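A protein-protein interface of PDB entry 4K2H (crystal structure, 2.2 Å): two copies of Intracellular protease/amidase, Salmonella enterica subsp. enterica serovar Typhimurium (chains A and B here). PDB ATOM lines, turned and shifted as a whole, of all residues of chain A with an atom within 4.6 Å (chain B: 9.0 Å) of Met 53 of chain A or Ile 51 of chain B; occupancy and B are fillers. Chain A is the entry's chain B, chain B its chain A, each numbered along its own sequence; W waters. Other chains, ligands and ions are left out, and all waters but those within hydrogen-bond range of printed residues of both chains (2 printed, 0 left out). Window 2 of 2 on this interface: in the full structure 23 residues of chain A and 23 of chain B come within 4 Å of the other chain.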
ATOM      1  N   PHE A  15     -21.757 -12.439   4.985  1.00  0.00           N
ATOM      2  CA  PHE A  15     -22.542 -13.573   4.588  1.00  0.00           C
ATOM      3  C   PHE A  15     -21.851 -14.876   4.981  1.00  0.00           C
ATOM      4  O   PHE A  15     -20.651 -15.027   4.870  1.00  0.00           O
ATOM      5  CB  PHE A  15     -22.846 -13.549   3.067  1.00  0.00           C
ATOM      6  CG  PHE A  15     -21.644 -13.843   2.171  1.00  0.00           C
ATOM      7  CD1 PHE A  15     -21.396 -15.134   1.719  1.00  0.00           C
ATOM      8  CD2 PHE A  15     -20.778 -12.832   1.780  1.00  0.00           C
ATOM      9  CE1 PHE A  15     -20.317 -15.407   0.908  1.00  0.00           C
ATOM     10  CE2 PHE A  15     -19.702 -13.094   0.967  1.00  0.00           C
ATOM     11  CZ  PHE A  15     -19.465 -14.383   0.533  1.00  0.00           C
ATOM     12  N   GLU A  17     -20.612 -17.938   4.010  1.00  0.00           N
ATOM     13  CA  GLU A  17     -20.219 -18.453   2.702  1.00  0.00           C
ATOM     14  C   GLU A  17     -20.606 -19.898   2.468  1.00  0.00           C
ATOM     15  O   GLU A  17     -20.911 -20.262   1.357  1.00  0.00           O
ATOM     16  CB  GLU A  17     -18.720 -18.268   2.479  1.00  0.00           C
ATOM     17  CG  GLU A  17     -17.763 -19.133   3.318  1.00  0.00           C
ATOM     18  CD  GLU A  17     -17.852 -18.918   4.795  1.00  0.00           C
ATOM     19  OE1 GLU A  17     -17.717 -17.761   5.262  1.00  0.00           O
ATOM     20  OE2 GLU A  17     -18.065 -19.955   5.495  1.00  0.00           O
ATOM     21  N   ILE A  21     -22.585 -20.830  -0.822  1.00  0.00           N
ATOM     22  CA  ILE A  21     -21.790 -21.535  -1.831  1.00  0.00           C
ATOM     23  C   ILE A  21     -22.359 -22.898  -2.174  1.00  0.00           C
ATOM     24  O   ILE A  21     -22.417 -23.277  -3.350  1.00  0.00           O
ATOM     25  CB  ILE A  21     -20.284 -21.602  -1.429  1.00  0.00           C
ATOM     26  CG1 ILE A  21     -19.536 -20.461  -2.101  1.00  0.00           C
ATOM     27  CG2 ILE A  21     -19.601 -22.879  -1.871  1.00  0.00           C
ATOM     28  CD1 ILE A  21     -20.189 -19.128  -1.843  1.00  0.00           C
ATOM     29  N   LEU A  24     -25.475 -22.346  -4.207  1.00  0.00           N
ATOM     30  CA  LEU A  24     -25.033 -21.944  -5.520  1.00  0.00           C
ATOM     31  C   LEU A  24     -24.429 -23.104  -6.312  1.00  0.00           C
ATOM     32  O   LEU A  24     -24.709 -23.281  -7.506  1.00  0.00           O
ATOM     33  CB  LEU A  24     -24.001 -20.849  -5.342  1.00  0.00           C
ATOM     34  CG  LEU A  24     -23.433 -20.216  -6.585  1.00  0.00           C
ATOM     35  CD1 LEU A  24     -23.133 -18.751  -6.255  1.00  0.00           C
ATOM     36  CD2 LEU A  24     -22.195 -20.973  -7.071  1.00  0.00           C
ATOM     37  N   ARG A  28     -25.991 -24.460  -9.860  1.00  0.00           N
ATOM     38  CA  ARG A  28     -25.165 -24.326 -11.074  1.00  0.00           C
ATOM     39  C   ARG A  28     -24.844 -25.692 -11.675  1.00  0.00           C
ATOM     40  O   ARG A  28     -24.710 -25.796 -12.889  1.00  0.00           O
ATOM     41  CB  ARG A  28     -23.894 -23.527 -10.828  1.00  0.00           C
ATOM     42  CG  ARG A  28     -24.164 -22.052 -10.687  1.00  0.00           C
ATOM     43  CD  ARG A  28     -22.906 -21.221 -10.876  1.00  0.00           C
ATOM     44  NE  ARG A  28     -23.268 -19.830 -11.027  1.00  0.00           N
ATOM     45  CZ  ARG A  28     -22.545 -18.800 -10.626  1.00  0.00           C
ATOM     46  NH1 ARG A  28     -21.400 -18.967 -10.001  1.00  0.00           N
ATOM     47  NH2 ARG A  28     -23.020 -17.577 -10.823  1.00  0.00           N
ATOM     48  N   ARG A  43     -18.216  -5.224  -6.190  1.00  0.00           N
ATOM     49  CA  ARG A  43     -18.487  -6.647  -6.311  1.00  0.00           C
ATOM     50  C   ARG A  43     -17.714  -7.440  -5.289  1.00  0.00           C
ATOM     51  O   ARG A  43     -17.996  -8.587  -5.069  1.00  0.00           O
ATOM     52  CB  ARG A  43     -18.150  -7.126  -7.713  1.00  0.00           C
ATOM     53  CG  ARG A  43     -19.076  -6.557  -8.777  1.00  0.00           C
ATOM     54  CD  ARG A  43     -18.702  -7.138 -10.132  1.00  0.00           C
ATOM     55  NE  ARG A  43     -19.483  -6.527 -11.197  1.00  0.00           N
ATOM     56  CZ  ARG A  43     -19.569  -6.985 -12.444  1.00  0.00           C
ATOM     57  NH1 ARG A  43     -18.900  -8.074 -12.817  1.00  0.00           N
ATOM     58  NH2 ARG A  43     -20.343  -6.340 -13.326  1.00  0.00           N
ATOM     59  N   ALA A  44     -16.736  -6.817  -4.676  1.00  0.00           N
ATOM     60  CA  ALA A  44     -15.968  -7.446  -3.619  1.00  0.00           C
ATOM     61  C   ALA A  44     -16.745  -7.434  -2.303  1.00  0.00           C
ATOM     62  O   ALA A  44     -17.217  -6.389  -1.818  1.00  0.00           O
ATOM     63  CB  ALA A  44     -14.619  -6.769  -3.449  1.00  0.00           C
ATOM     64  N   VAL A  45     -16.905  -8.628  -1.779  1.00  0.00           N
ATOM     65  CA  VAL A  45     -17.591  -8.862  -0.505  1.00  0.00           C
ATOM     66  C   VAL A  45     -16.858  -9.974   0.226  1.00  0.00           C
ATOM     67  O   VAL A  45     -16.465 -10.994  -0.382  1.00  0.00           O
ATOM     68  CB  VAL A  45     -19.045  -9.312  -0.708  1.00  0.00           C
ATOM     69  CG1 VAL A  45     -19.737  -9.557   0.628  1.00  0.00           C
ATOM     70  CG2 VAL A  45     -19.819  -8.291  -1.511  1.00  0.00           C
ATOM     71  N   ILE A  51     -13.472 -14.998   3.767  1.00  0.00           N
ATOM     72  CA  ILE A  51     -13.131 -15.249   2.378  1.00  0.00           C
ATOM     73  C   ILE A  51     -13.639 -14.102   1.532  1.00  0.00           C
ATOM     74  O   ILE A  51     -14.835 -13.915   1.437  1.00  0.00           O
ATOM     75  CB  ILE A  51     -13.757 -16.535   1.853  1.00  0.00           C
ATOM     76  CG1 ILE A  51     -13.365 -17.682   2.756  1.00  0.00           C
ATOM     77  CG2 ILE A  51     -13.263 -16.773   0.436  1.00  0.00           C
ATOM     78  CD1 ILE A  51     -13.788 -19.033   2.240  1.00  0.00           C
ATOM     79  N   PRO A  52     -12.725 -13.332   0.927  1.00  0.00           N
ATOM     80  CA  PRO A  52     -13.131 -12.332  -0.070  1.00  0.00           C
ATOM     81  C   PRO A  52     -13.526 -13.002  -1.372  1.00  0.00           C
ATOM     82  O   PRO A  52     -12.798 -13.845  -1.844  1.00  0.00           O
ATOM     83  CB  PRO A  52     -11.882 -11.466  -0.248  1.00  0.00           C
ATOM     84  CG  PRO A  52     -10.871 -11.941   0.804  1.00  0.00           C
ATOM     85  CD  PRO A  52     -11.271 -13.350   1.136  1.00  0.00           C
ATOM     86  N   MET A  53     -14.688 -12.646  -1.923  1.00  0.00           N
ATOM     87  CA  MET A  53     -15.187 -13.207  -3.168  1.00  0.00           C
ATOM     88  C   MET A  53     -15.637 -12.088  -4.063  1.00  0.00           C
ATOM     89  O   MET A  53     -15.920 -10.999  -3.585  1.00  0.00           O
ATOM     90  CB  MET A  53     -16.414 -14.108  -2.917  1.00  0.00           C
ATOM     91  CG  MET A  53     -16.170 -15.251  -1.976  1.00  0.00           C
ATOM     92  SD  MET A  53     -17.432 -16.500  -1.874  1.00  0.00           S
ATOM     93  CE  MET A  53     -16.773 -17.405  -0.458  1.00  0.00           C
ATOM     94  N   VAL A  54     -15.755 -12.360  -5.361  1.00  0.00           N
ATOM     95  CA  VAL A  54     -16.243 -11.356  -6.297  1.00  0.00           C
ATOM     96  C   VAL A  54     -17.574 -11.774  -6.835  1.00  0.00           C
ATOM     97  O   VAL A  54     -17.688 -12.784  -7.504  1.00  0.00           O
ATOM     98  CB  VAL A  54     -15.277 -11.120  -7.479  1.00  0.00           C
ATOM     99  CG1 VAL A  54     -15.883 -10.155  -8.485  1.00  0.00           C
ATOM    100  CG2 VAL A  54     -13.945 -10.593  -6.974  1.00  0.00           C
ATOM    101  N   ALA A  55     -18.579 -10.980  -6.530  1.00  0.00           N
ATOM    102  CA  ALA A  55     -19.921 -11.235  -6.968  1.00  0.00           C
ATOM    103  C   ALA A  55     -20.022 -11.052  -8.461  1.00  0.00           C
ATOM    104  O   ALA A  55     -19.216 -10.369  -9.050  1.00  0.00           O
ATOM    105  CB  ALA A  55     -20.858 -10.269  -6.260  1.00  0.00           C
ATOM    106  N   LEU B  11      -5.813 -24.149  -3.379  1.00  0.00           N
ATOM    107  CA  LEU B  11      -6.804 -23.667  -4.323  1.00  0.00           C
ATOM    108  C   LEU B  11      -6.206 -23.495  -5.716  1.00  0.00           C
ATOM    109  O   LEU B  11      -5.587 -22.487  -5.987  1.00  0.00           O
ATOM    110  CB  LEU B  11      -7.397 -22.344  -3.838  1.00  0.00           C
ATOM    111  CG  LEU B  11      -8.138 -22.328  -2.506  1.00  0.00           C
ATOM    112  CD1 LEU B  11      -8.809 -20.972  -2.299  1.00  0.00           C
ATOM    113  CD2 LEU B  11      -9.165 -23.455  -2.372  1.00  0.00           C
ATOM    114  N   ALA B  12      -6.429 -24.451  -6.607  1.00  0.00           N
ATOM    115  CA  ALA B  12      -5.976 -24.318  -7.991  1.00  0.00           C
ATOM    116  C   ALA B  12      -7.140 -23.810  -8.868  1.00  0.00           C
ATOM    117  O   ALA B  12      -8.292 -23.883  -8.452  1.00  0.00           O
ATOM    118  CB  ALA B  12      -5.452 -25.646  -8.504  1.00  0.00           C
ATOM    119  N   PRO B  13      -6.852 -23.305 -10.084  1.00  0.00           N
ATOM    120  CA  PRO B  13      -7.988 -22.848 -10.910  1.00  0.00           C
ATOM    121  C   PRO B  13      -8.931 -23.993 -11.166  1.00  0.00           C
ATOM    122  O   PRO B  13      -8.476 -25.097 -11.486  1.00  0.00           O
ATOM    123  CB  PRO B  13      -7.301 -22.307 -12.205  1.00  0.00           C
ATOM    124  CG  PRO B  13      -5.965 -21.844 -11.715  1.00  0.00           C
ATOM    125  CD  PRO B  13      -5.568 -22.880 -10.670  1.00  0.00           C
ATOM    126  N   GLY B  14     -10.230 -23.758 -10.984  1.00  0.00           N
ATOM    127  CA  GLY B  14     -11.200 -24.840 -11.103  1.00  0.00           C
ATOM    128  C   GLY B  14     -11.462 -25.699  -9.868  1.00  0.00           C
ATOM    129  O   GLY B  14     -12.158 -26.666  -9.937  1.00  0.00           O
ATOM    130  N   PHE B  15     -10.932 -25.315  -8.730  1.00  0.00           N
ATOM    131  CA  PHE B  15     -11.167 -26.029  -7.471  1.00  0.00           C
ATOM    132  C   PHE B  15     -12.650 -26.074  -7.196  1.00  0.00           C
ATOM    133  O   PHE B  15     -13.345 -25.126  -7.496  1.00  0.00           O
ATOM    134  CB  PHE B  15     -10.429 -25.341  -6.309  1.00  0.00           C
ATOM    135  CG  PHE B  15     -11.001 -23.990  -5.879  1.00  0.00           C
ATOM    136  CD1 PHE B  15     -11.852 -23.894  -4.790  1.00  0.00           C
ATOM    137  CD2 PHE B  15     -10.664 -22.816  -6.544  1.00  0.00           C
ATOM    138  CE1 PHE B  15     -12.354 -22.688  -4.353  1.00  0.00           C
ATOM    139  CE2 PHE B  15     -11.178 -21.593  -6.139  1.00  0.00           C
ATOM    140  CZ  PHE B  15     -11.998 -21.524  -5.014  1.00  0.00           C
ATOM    141  N   GLU B  16     -13.125 -27.187  -6.610  1.00  0.00           N
ATOM    142  CA  GLU B  16     -14.505 -27.347  -6.287  1.00  0.00           C
ATOM    143  C   GLU B  16     -14.758 -26.518  -5.045  1.00  0.00           C
ATOM    144  O   GLU B  16     -14.286 -26.857  -3.964  1.00  0.00           O
ATOM    145  CB  GLU B  16     -14.852 -28.825  -6.044  1.00  0.00           C
ATOM    146  CG  GLU B  16     -16.186 -29.250  -6.621  1.00  0.00           C
ATOM    147  CD  GLU B  16     -17.261 -28.192  -6.424  1.00  0.00           C
ATOM    148  OE1 GLU B  16     -17.848 -27.744  -7.446  1.00  0.00           O
ATOM    149  OE2 GLU B  16     -17.485 -27.778  -5.253  1.00  0.00           O
ATOM    150  N   GLU B  17     -15.508 -25.420  -5.205  1.00  0.00           N
ATOM    151  CA  GLU B  17     -15.676 -24.462  -4.131  1.00  0.00           C
ATOM    152  C   GLU B  17     -16.488 -24.977  -2.970  1.00  0.00           C
ATOM    153  O   GLU B  17     -16.223 -24.630  -1.831  1.00  0.00           O
ATOM    154  CB  GLU B  17     -16.230 -23.142  -4.635  1.00  0.00           C
ATOM    155  CG  GLU B  17     -17.680 -23.112  -5.126  1.00  0.00           C
ATOM    156  CD  GLU B  17     -17.967 -24.004  -6.305  1.00  0.00           C
ATOM    157  OE1 GLU B  17     -17.213 -23.930  -7.286  1.00  0.00           O
ATOM    158  OE2 GLU B  17     -18.954 -24.800  -6.218  1.00  0.00           O
ATOM    159  N   ALA B  18     -17.490 -25.791  -3.254  1.00  0.00           N
ATOM    160  CA  ALA B  18     -18.350 -26.276  -2.189  1.00  0.00           C
ATOM    161  C   ALA B  18     -17.547 -27.195  -1.242  1.00  0.00           C
ATOM    162  O   ALA B  18     -17.639 -27.071  -0.015  1.00  0.00           O
ATOM    163  CB  ALA B  18     -19.566 -26.969  -2.777  1.00  0.00           C
ATOM    164  N   ALA B  20     -14.158 -27.287  -0.738  1.00  0.00           N
ATOM    165  CA  ALA B  20     -13.242 -26.431  -0.046  1.00  0.00           C
ATOM    166  C   ALA B  20     -13.902 -25.508   0.966  1.00  0.00           C
ATOM    167  O   ALA B  20     -13.402 -25.341   2.086  1.00  0.00           O
ATOM    168  CB  ALA B  20     -12.460 -25.586  -1.049  1.00  0.00           C
ATOM    169  N   ILE B  21     -14.985 -24.851   0.576  1.00  0.00           N
ATOM    170  CA  ILE B  21     -15.582 -23.872   1.491  1.00  0.00           C
ATOM    171  C   ILE B  21     -16.257 -24.507   2.712  1.00  0.00           C
ATOM    172  O   ILE B  21     -16.144 -23.946   3.804  1.00  0.00           O
ATOM    173  CB  ILE B  21     -16.560 -22.902   0.789  1.00  0.00           C
ATOM    174  CG1 ILE B  21     -15.829 -21.894  -0.111  1.00  0.00           C
ATOM    175  CG2 ILE B  21     -17.395 -22.150   1.802  1.00  0.00           C
ATOM    176  CD1 ILE B  21     -14.310 -21.921  -0.044  1.00  0.00           C
ATOM    177  N   VAL B  22     -16.945 -25.646   2.550  1.00  0.00           N
ATOM    178  CA  VAL B  22     -17.568 -26.297   3.718  1.00  0.00           C
ATOM    179  C   VAL B  22     -16.453 -26.724   4.677  1.00  0.00           C
ATOM    180  O   VAL B  22     -16.554 -26.482   5.877  1.00  0.00           O
ATOM    181  CB  VAL B  22     -18.515 -27.457   3.355  1.00  0.00           C
ATOM    182  CG1 VAL B  22     -19.054 -28.162   4.605  1.00  0.00           C
ATOM    183  CG2 VAL B  22     -19.705 -26.960   2.562  1.00  0.00           C
ATOM    184  N   LEU B  24     -13.463 -25.478   5.042  1.00  0.00           N
ATOM    185  CA  LEU B  24     -12.912 -24.303   5.652  1.00  0.00           C
ATOM    186  C   LEU B  24     -13.851 -23.736   6.724  1.00  0.00           C
ATOM    187  O   LEU B  24     -13.427 -23.337   7.803  1.00  0.00           O
ATOM    188  CB  LEU B  24     -12.639 -23.289   4.547  1.00  0.00           C
ATOM    189  CG  LEU B  24     -12.023 -22.021   5.031  1.00  0.00           C
ATOM    190  CD1 LEU B  24     -11.088 -21.526   3.940  1.00  0.00           C
ATOM    191  CD2 LEU B  24     -13.121 -21.033   5.415  1.00  0.00           C
ATOM    192  N   ARG B  28     -12.864 -23.456  10.679  1.00  0.00           N
ATOM    193  CA  ARG B  28     -12.815 -22.133  11.281  1.00  0.00           C
ATOM    194  C   ARG B  28     -13.871 -21.962  12.376  1.00  0.00           C
ATOM    195  O   ARG B  28     -13.664 -21.176  13.290  1.00  0.00           O
ATOM    196  CB  ARG B  28     -12.896 -20.994  10.217  1.00  0.00           C
ATOM    197  CG  ARG B  28     -11.531 -20.590   9.666  1.00  0.00           C
ATOM    198  CD  ARG B  28     -11.569 -19.557   8.521  1.00  0.00           C
ATOM    199  NE  ARG B  28     -10.240 -19.309   7.926  1.00  0.00           N
ATOM    200  CZ  ARG B  28      -9.988 -18.728   6.746  1.00  0.00           C
ATOM    201  NH1 ARG B  28     -10.956 -18.297   5.929  1.00  0.00           N
ATOM    202  NH2 ARG B  28      -8.727 -18.610   6.347  1.00  0.00           N
ATOM    203  N   ALA B  44      -5.941 -14.343  -6.512  1.00  0.00           N
ATOM    204  CA  ALA B  44      -7.319 -14.544  -6.972  1.00  0.00           C
ATOM    205  C   ALA B  44      -7.383 -15.869  -7.698  1.00  0.00           C
ATOM    206  O   ALA B  44      -6.536 -16.158  -8.519  1.00  0.00           O
ATOM    207  CB  ALA B  44      -7.762 -13.418  -7.885  1.00  0.00           C
ATOM    208  N   VAL B  45      -8.375 -16.693  -7.378  1.00  0.00           N
ATOM    209  CA  VAL B  45      -8.535 -17.977  -8.060  1.00  0.00           C
ATOM    210  C   VAL B  45     -10.005 -18.204  -8.332  1.00  0.00           C
ATOM    211  O   VAL B  45     -10.848 -18.015  -7.436  1.00  0.00           O
ATOM    212  CB  VAL B  45      -8.058 -19.135  -7.174  1.00  0.00           C
ATOM    213  CG1 VAL B  45      -8.034 -20.423  -7.970  1.00  0.00           C
ATOM    214  CG2 VAL B  45      -6.688 -18.854  -6.587  1.00  0.00           C
ATOM    215  N   VAL B  46     -10.321 -18.645  -9.535  1.00  0.00           N
ATOM    216  CA  VAL B  46     -11.708 -18.880  -9.899  1.00  0.00           C
ATOM    217  C   VAL B  46     -12.070 -20.379  -9.777  1.00  0.00           C
ATOM    218  O   VAL B  46     -11.408 -21.247 -10.364  1.00  0.00           O
ATOM    219  CB  VAL B  46     -11.978 -18.337 -11.315  1.00  0.00           C
ATOM    220  CG1 VAL B  46     -13.416 -18.579 -11.748  1.00  0.00           C
ATOM    221  CG2 VAL B  46     -11.692 -16.855 -11.341  1.00  0.00           C
ATOM    222  N   SER B  47     -13.107 -20.662  -8.998  1.00  0.00           N
ATOM    223  CA  SER B  47     -13.548 -22.035  -8.734  1.00  0.00           C
ATOM    224  C   SER B  47     -14.229 -22.699  -9.935  1.00  0.00           C
ATOM    225  O   SER B  47     -14.608 -22.036 -10.944  1.00  0.00           O
ATOM    226  CB  SER B  47     -14.555 -22.041  -7.569  1.00  0.00           C
ATOM    227  OG  SER B  47     -15.880 -21.672  -8.023  1.00  0.00           O
ATOM    228  N   TYR B  48     -14.453 -24.005  -9.792  1.00  0.00           N
ATOM    229  CA  TYR B  48     -15.182 -24.816 -10.788  1.00  0.00           C
ATOM    230  C   TYR B  48     -16.498 -24.179 -11.209  1.00  0.00           C
ATOM    231  O   TYR B  48     -16.797 -24.101 -12.381  1.00  0.00           O
ATOM    232  CB  TYR B  48     -15.458 -26.203 -10.193  1.00  0.00           C
ATOM    233  CG  TYR B  48     -16.198 -27.208 -11.061  1.00  0.00           C
ATOM    234  CD1 TYR B  48     -16.134 -27.183 -12.463  1.00  0.00           C
ATOM    235  CD2 TYR B  48     -16.914 -28.239 -10.453  1.00  0.00           C
ATOM    236  CE1 TYR B  48     -16.798 -28.140 -13.227  1.00  0.00           C
ATOM    237  CE2 TYR B  48     -17.572 -29.190 -11.184  1.00  0.00           C
ATOM    238  CZ  TYR B  48     -17.527 -29.138 -12.559  1.00  0.00           C
ATOM    239  OH  TYR B  48     -18.215 -30.111 -13.232  1.00  0.00           O
ATOM    240  N   HIS B  49     -17.307 -23.778 -10.237  1.00  0.00           N
ATOM    241  CA  HIS B  49     -18.581 -23.106 -10.509  1.00  0.00           C
ATOM    242  C   HIS B  49     -18.480 -21.572 -10.514  1.00  0.00           C
ATOM    243  O   HIS B  49     -19.416 -20.881 -10.152  1.00  0.00           O
ATOM    244  CB  HIS B  49     -19.673 -23.647  -9.579  1.00  0.00           C
ATOM    245  CG  HIS B  49     -20.035 -25.070  -9.890  1.00  0.00           C
ATOM    246  ND1 HIS B  49     -19.802 -26.110  -9.021  1.00  0.00           N
ATOM    247  CD2 HIS B  49     -20.551 -25.629 -11.012  1.00  0.00           C
ATOM    248  CE1 HIS B  49     -20.135 -27.245  -9.600  1.00  0.00           C
ATOM    249  NE2 HIS B  49     -20.617 -26.980 -10.796  1.00  0.00           N
ATOM    250  N   ASP B  50     -17.345 -21.074 -10.982  1.00  0.00           N
ATOM    251  CA  ASP B  50     -17.121 -19.679 -11.325  1.00  0.00           C
ATOM    252  C   ASP B  50     -17.180 -18.672 -10.213  1.00  0.00           C
ATOM    253  O   ASP B  50     -17.593 -17.551 -10.441  1.00  0.00           O
ATOM    254  CB  ASP B  50     -18.084 -19.226 -12.418  1.00  0.00           C
ATOM    255  CG  ASP B  50     -17.802 -19.880 -13.716  1.00  0.00           C
ATOM    256  OD1 ASP B  50     -16.595 -20.018 -14.052  1.00  0.00           O
ATOM    257  OD2 ASP B  50     -18.785 -20.253 -14.405  1.00  0.00           O
ATOM    258  N   ILE B  51     -16.726 -19.024  -9.026  1.00  0.00           N
ATOM    259  CA  ILE B  51     -16.653 -18.037  -7.973  1.00  0.00           C
ATOM    260  C   ILE B  51     -15.223 -17.623  -7.794  1.00  0.00           C
ATOM    261  O   ILE B  51     -14.386 -18.468  -7.575  1.00  0.00           O
ATOM    262  CB  ILE B  51     -17.196 -18.544  -6.650  1.00  0.00           C
ATOM    263  CG1 ILE B  51     -18.629 -19.004  -6.863  1.00  0.00           C
ATOM    264  CG2 ILE B  51     -17.159 -17.394  -5.637  1.00  0.00           C
ATOM    265  CD1 ILE B  51     -19.180 -19.735  -5.678  1.00  0.00           C
ATOM    266  N   PRO B  52     -14.946 -16.321  -7.962  1.00  0.00           N
ATOM    267  CA  PRO B  52     -13.585 -15.909  -7.737  1.00  0.00           C
ATOM    268  C   PRO B  52     -13.398 -15.630  -6.275  1.00  0.00           C
ATOM    269  O   PRO B  52     -14.252 -14.982  -5.653  1.00  0.00           O
ATOM    270  CB  PRO B  52     -13.435 -14.619  -8.553  1.00  0.00           C
ATOM    271  CG  PRO B  52     -14.694 -14.496  -9.373  1.00  0.00           C
ATOM    272  CD  PRO B  52     -15.734 -15.278  -8.639  1.00  0.00           C
ATOM    273  N   MET B  53     -12.282 -16.109  -5.755  1.00  0.00           N
ATOM    274  CA  MET B  53     -11.934 -15.956  -4.352  1.00  0.00           C
ATOM    275  C   MET B  53     -10.497 -15.549  -4.198  1.00  0.00           C
ATOM    276  O   MET B  53      -9.623 -16.028  -4.901  1.00  0.00           O
ATOM    277  CB  MET B  53     -12.074 -17.251  -3.604  1.00  0.00           C
ATOM    278  CG  MET B  53     -13.419 -17.844  -3.759  1.00  0.00           C
ATOM    279  SD  MET B  53     -13.707 -19.225  -2.598  1.00  0.00           S
ATOM    280  CE  MET B  53     -15.319 -19.650  -3.181  1.00  0.00           C
ATOM    281  N   VAL B  54     -10.243 -14.720  -3.214  1.00  0.00           N
ATOM    282  CA  VAL B  54      -8.887 -14.340  -2.924  1.00  0.00           C
ATOM    283  C   VAL B  54      -8.325 -15.271  -1.852  1.00  0.00           C
ATOM    284  O   VAL B  54      -8.725 -15.180  -0.701  1.00  0.00           O
ATOM    285  CB  VAL B  54      -8.840 -12.883  -2.447  1.00  0.00           C
ATOM    286  CG1 VAL B  54      -7.410 -12.474  -2.179  1.00  0.00           C
ATOM    287  CG2 VAL B  54      -9.514 -11.972  -3.469  1.00  0.00           C
ATOM    288  N   ALA B  55      -7.381 -16.135  -2.234  1.00  0.00           N
ATOM    289  CA  ALA B  55      -6.612 -16.921  -1.250  1.00  0.00           C
ATOM    290  C   ALA B  55      -5.869 -16.085  -0.214  1.00  0.00           C
ATOM    291  O   ALA B  55      -5.429 -14.959  -0.473  1.00  0.00           O
ATOM    292  CB  ALA B  55      -5.639 -17.884  -1.944  1.00  0.00           C
HETATM  293  O   HOH W   1     -19.827 -16.343  -9.581  1.00  0.00           O
HETATM  294  O   HOH W   2     -21.400 -19.572 -13.936  1.00  0.00           O
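Of the 25 printed residues of chain B, 9 touch a printed residue of chain A.
Printed residues of chain B that touch a printed residue of chain A: Glu 17, Ala 18, Ile 21, Leu 24, His 49, Ile 51, Pro 52, Met 53 and Val 54.
Hydrophobic or aromatic side chains of chain B within 4 Å of the printed part of chain A: Ile 21, Leu 24, His 49, Ile 51, Pro 52, Met 53 and Val 54.
Of the 13 printed residues of chain A, 8 touch a printed residue of chain B.
Printed residues of chain A that touch a printed residue of chain B: Glu 17, Ile 21, Leu 24, Arg 28, Ile 51, Pro 52, Met 53 and Val 54.
Hydrophobic or aromatic side chains of chain A within 4 Å of the printed part of chain B: Ile 21, Leu 24, Ile 51, Pro 52, Met 53 and Val 54.
Along chain A the printed residues that touch a printed residue of chain B span positions 17 to 54.
Among the printed residues, 15 pairs touch across the chains.
Among the printed residues, no Asp or Glu carboxylate lies within 4 Å of a Lys or Arg side-chain nitrogen of the other chain.
Phe 15 of chain A touches none of the printed residues of chain B.
Of the printed residues of chain B, Leu 24 of chain A touches Ile 51 (3.5 Å).
Met 53 of chain A touches three residues of chain B.
Of chain B, only Pro 52 (3.0 Å) comes within 4 Å of Val 54 of chain A.
Val 46 of chain B touches none of the printed residues of chain A.
Of the printed residues of chain A, His 49 of chain B touches Arg 28.
Of chain A, only Ile 21, Leu 24 and Met 53 come within 4 Å of Ile 51 of chain B.
Of the printed residues of chain A, Pro 52 of chain B touches Met 53 (3.2 Å) and Val 54 (3.0 Å).
Printed residues of chain A within 4 Å of Met 53 of chain B: Ile 51 (3.9 Å), Pro 52 (3.4 Å) and Met 53 (3.8 Å).
The nearest residue of chain B that does not touch Met 53 of chain A is Ile 21 of chain B (4.6 Å).
The nearest residue of chain A that does not touch Ile 51 of chain B is Arg 28 of chain A (4.2 Å).
The nearest printed residue of chain B that does not touch Ile 21 of chain A is Ile 21 of chain B (4.04 Å).
Water W1 lies within hydrogen-bond range of O of Asp 50 of chain B (2.7 Å) and NH1 of Arg 28 of chain A (3.1 Å).
Water W2 bridges the side-chain carboxylate (OD2) of Asp 50 of chain B and the guanidinium group (NE) of Arg 28 of chain A.
Ile 21 of chain B touches Glu 17 of chain A (CG2 to CG, 3.4 Å).
Glu 17 of chain B touches Ile 21 of chain A.
Ala 18 of chain B touches Ile 21 of chain A.
Ile 51 of chain B touches Leu 24 of chain A.
Ile 51 of chain A touches Ile 21 of chain B (CD1 to CD1, 3.7 Å).
Ile 51 of chain A touches Leu 24 of chain B.
Met 53 of chain B touches Ile 51 of chain A.
SD of Met 53 of chain A touches CG2 of Ile 51 of chain B, 3.9 Å away.
Met 53 of chain B touches Met 53 of chain A (CE to CE, 3.8 Å).
Ile 21 of chain A touches Ile 51 of chain B, and with the chains exchanged Ile 51 of chain A touches Ile 21 of chain B.
Ile 51 of chain A touches Met 53 of chain B, and with the chains exchanged Met 53 of chain A touches Ile 51 of chain B.
Positions printed for both chains: 15, 17, 21, 24, 28, 44, 45, 51, 52, 53, 54 and 55.
Of the 15 pairs that touch across the chains among the printed residues, 13 have their exchanged pair printed and touching as well.
The backbone carbonyl oxygen of His 49 of chain B sits at hydrogen-bond distance from the guanidinium group of Arg 28 of chain A (2.8 Å).
The backbone carbonyl oxygen of Pro 52 of chain B sits at hydrogen-bond distance from the backbone NH of Val 54 of chain A (3.0 Å).
The backbone carbonyl oxygen (O) of Pro 52 of chain A lies within hydrogen-bond range of the backbone NH (N) of Val 54 of chain B, 3.0 Å away.
OE2 of Glu 16 of chain B is in hydrogen-bond range of N of Ala 18 of chain B, at 2.8 Å.
The side-chain hydroxyl (OG) of Ser 47 of chain B lies within hydrogen-bond range of the side-chain carboxylate (OE1) of Glu 17 of chain B, at 2.7 Å.
The side-chain hydroxyl (OG) of Ser 47 of chain B sits close to the backbone NH (N) of His 49 of chain B (3.4 Å).
The side-chain hydroxyl (OG) of Ser 47 of chain B sits at hydrogen-bond distance from the backbone NH (N) of Ile 51 of chain B (3.0 Å).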
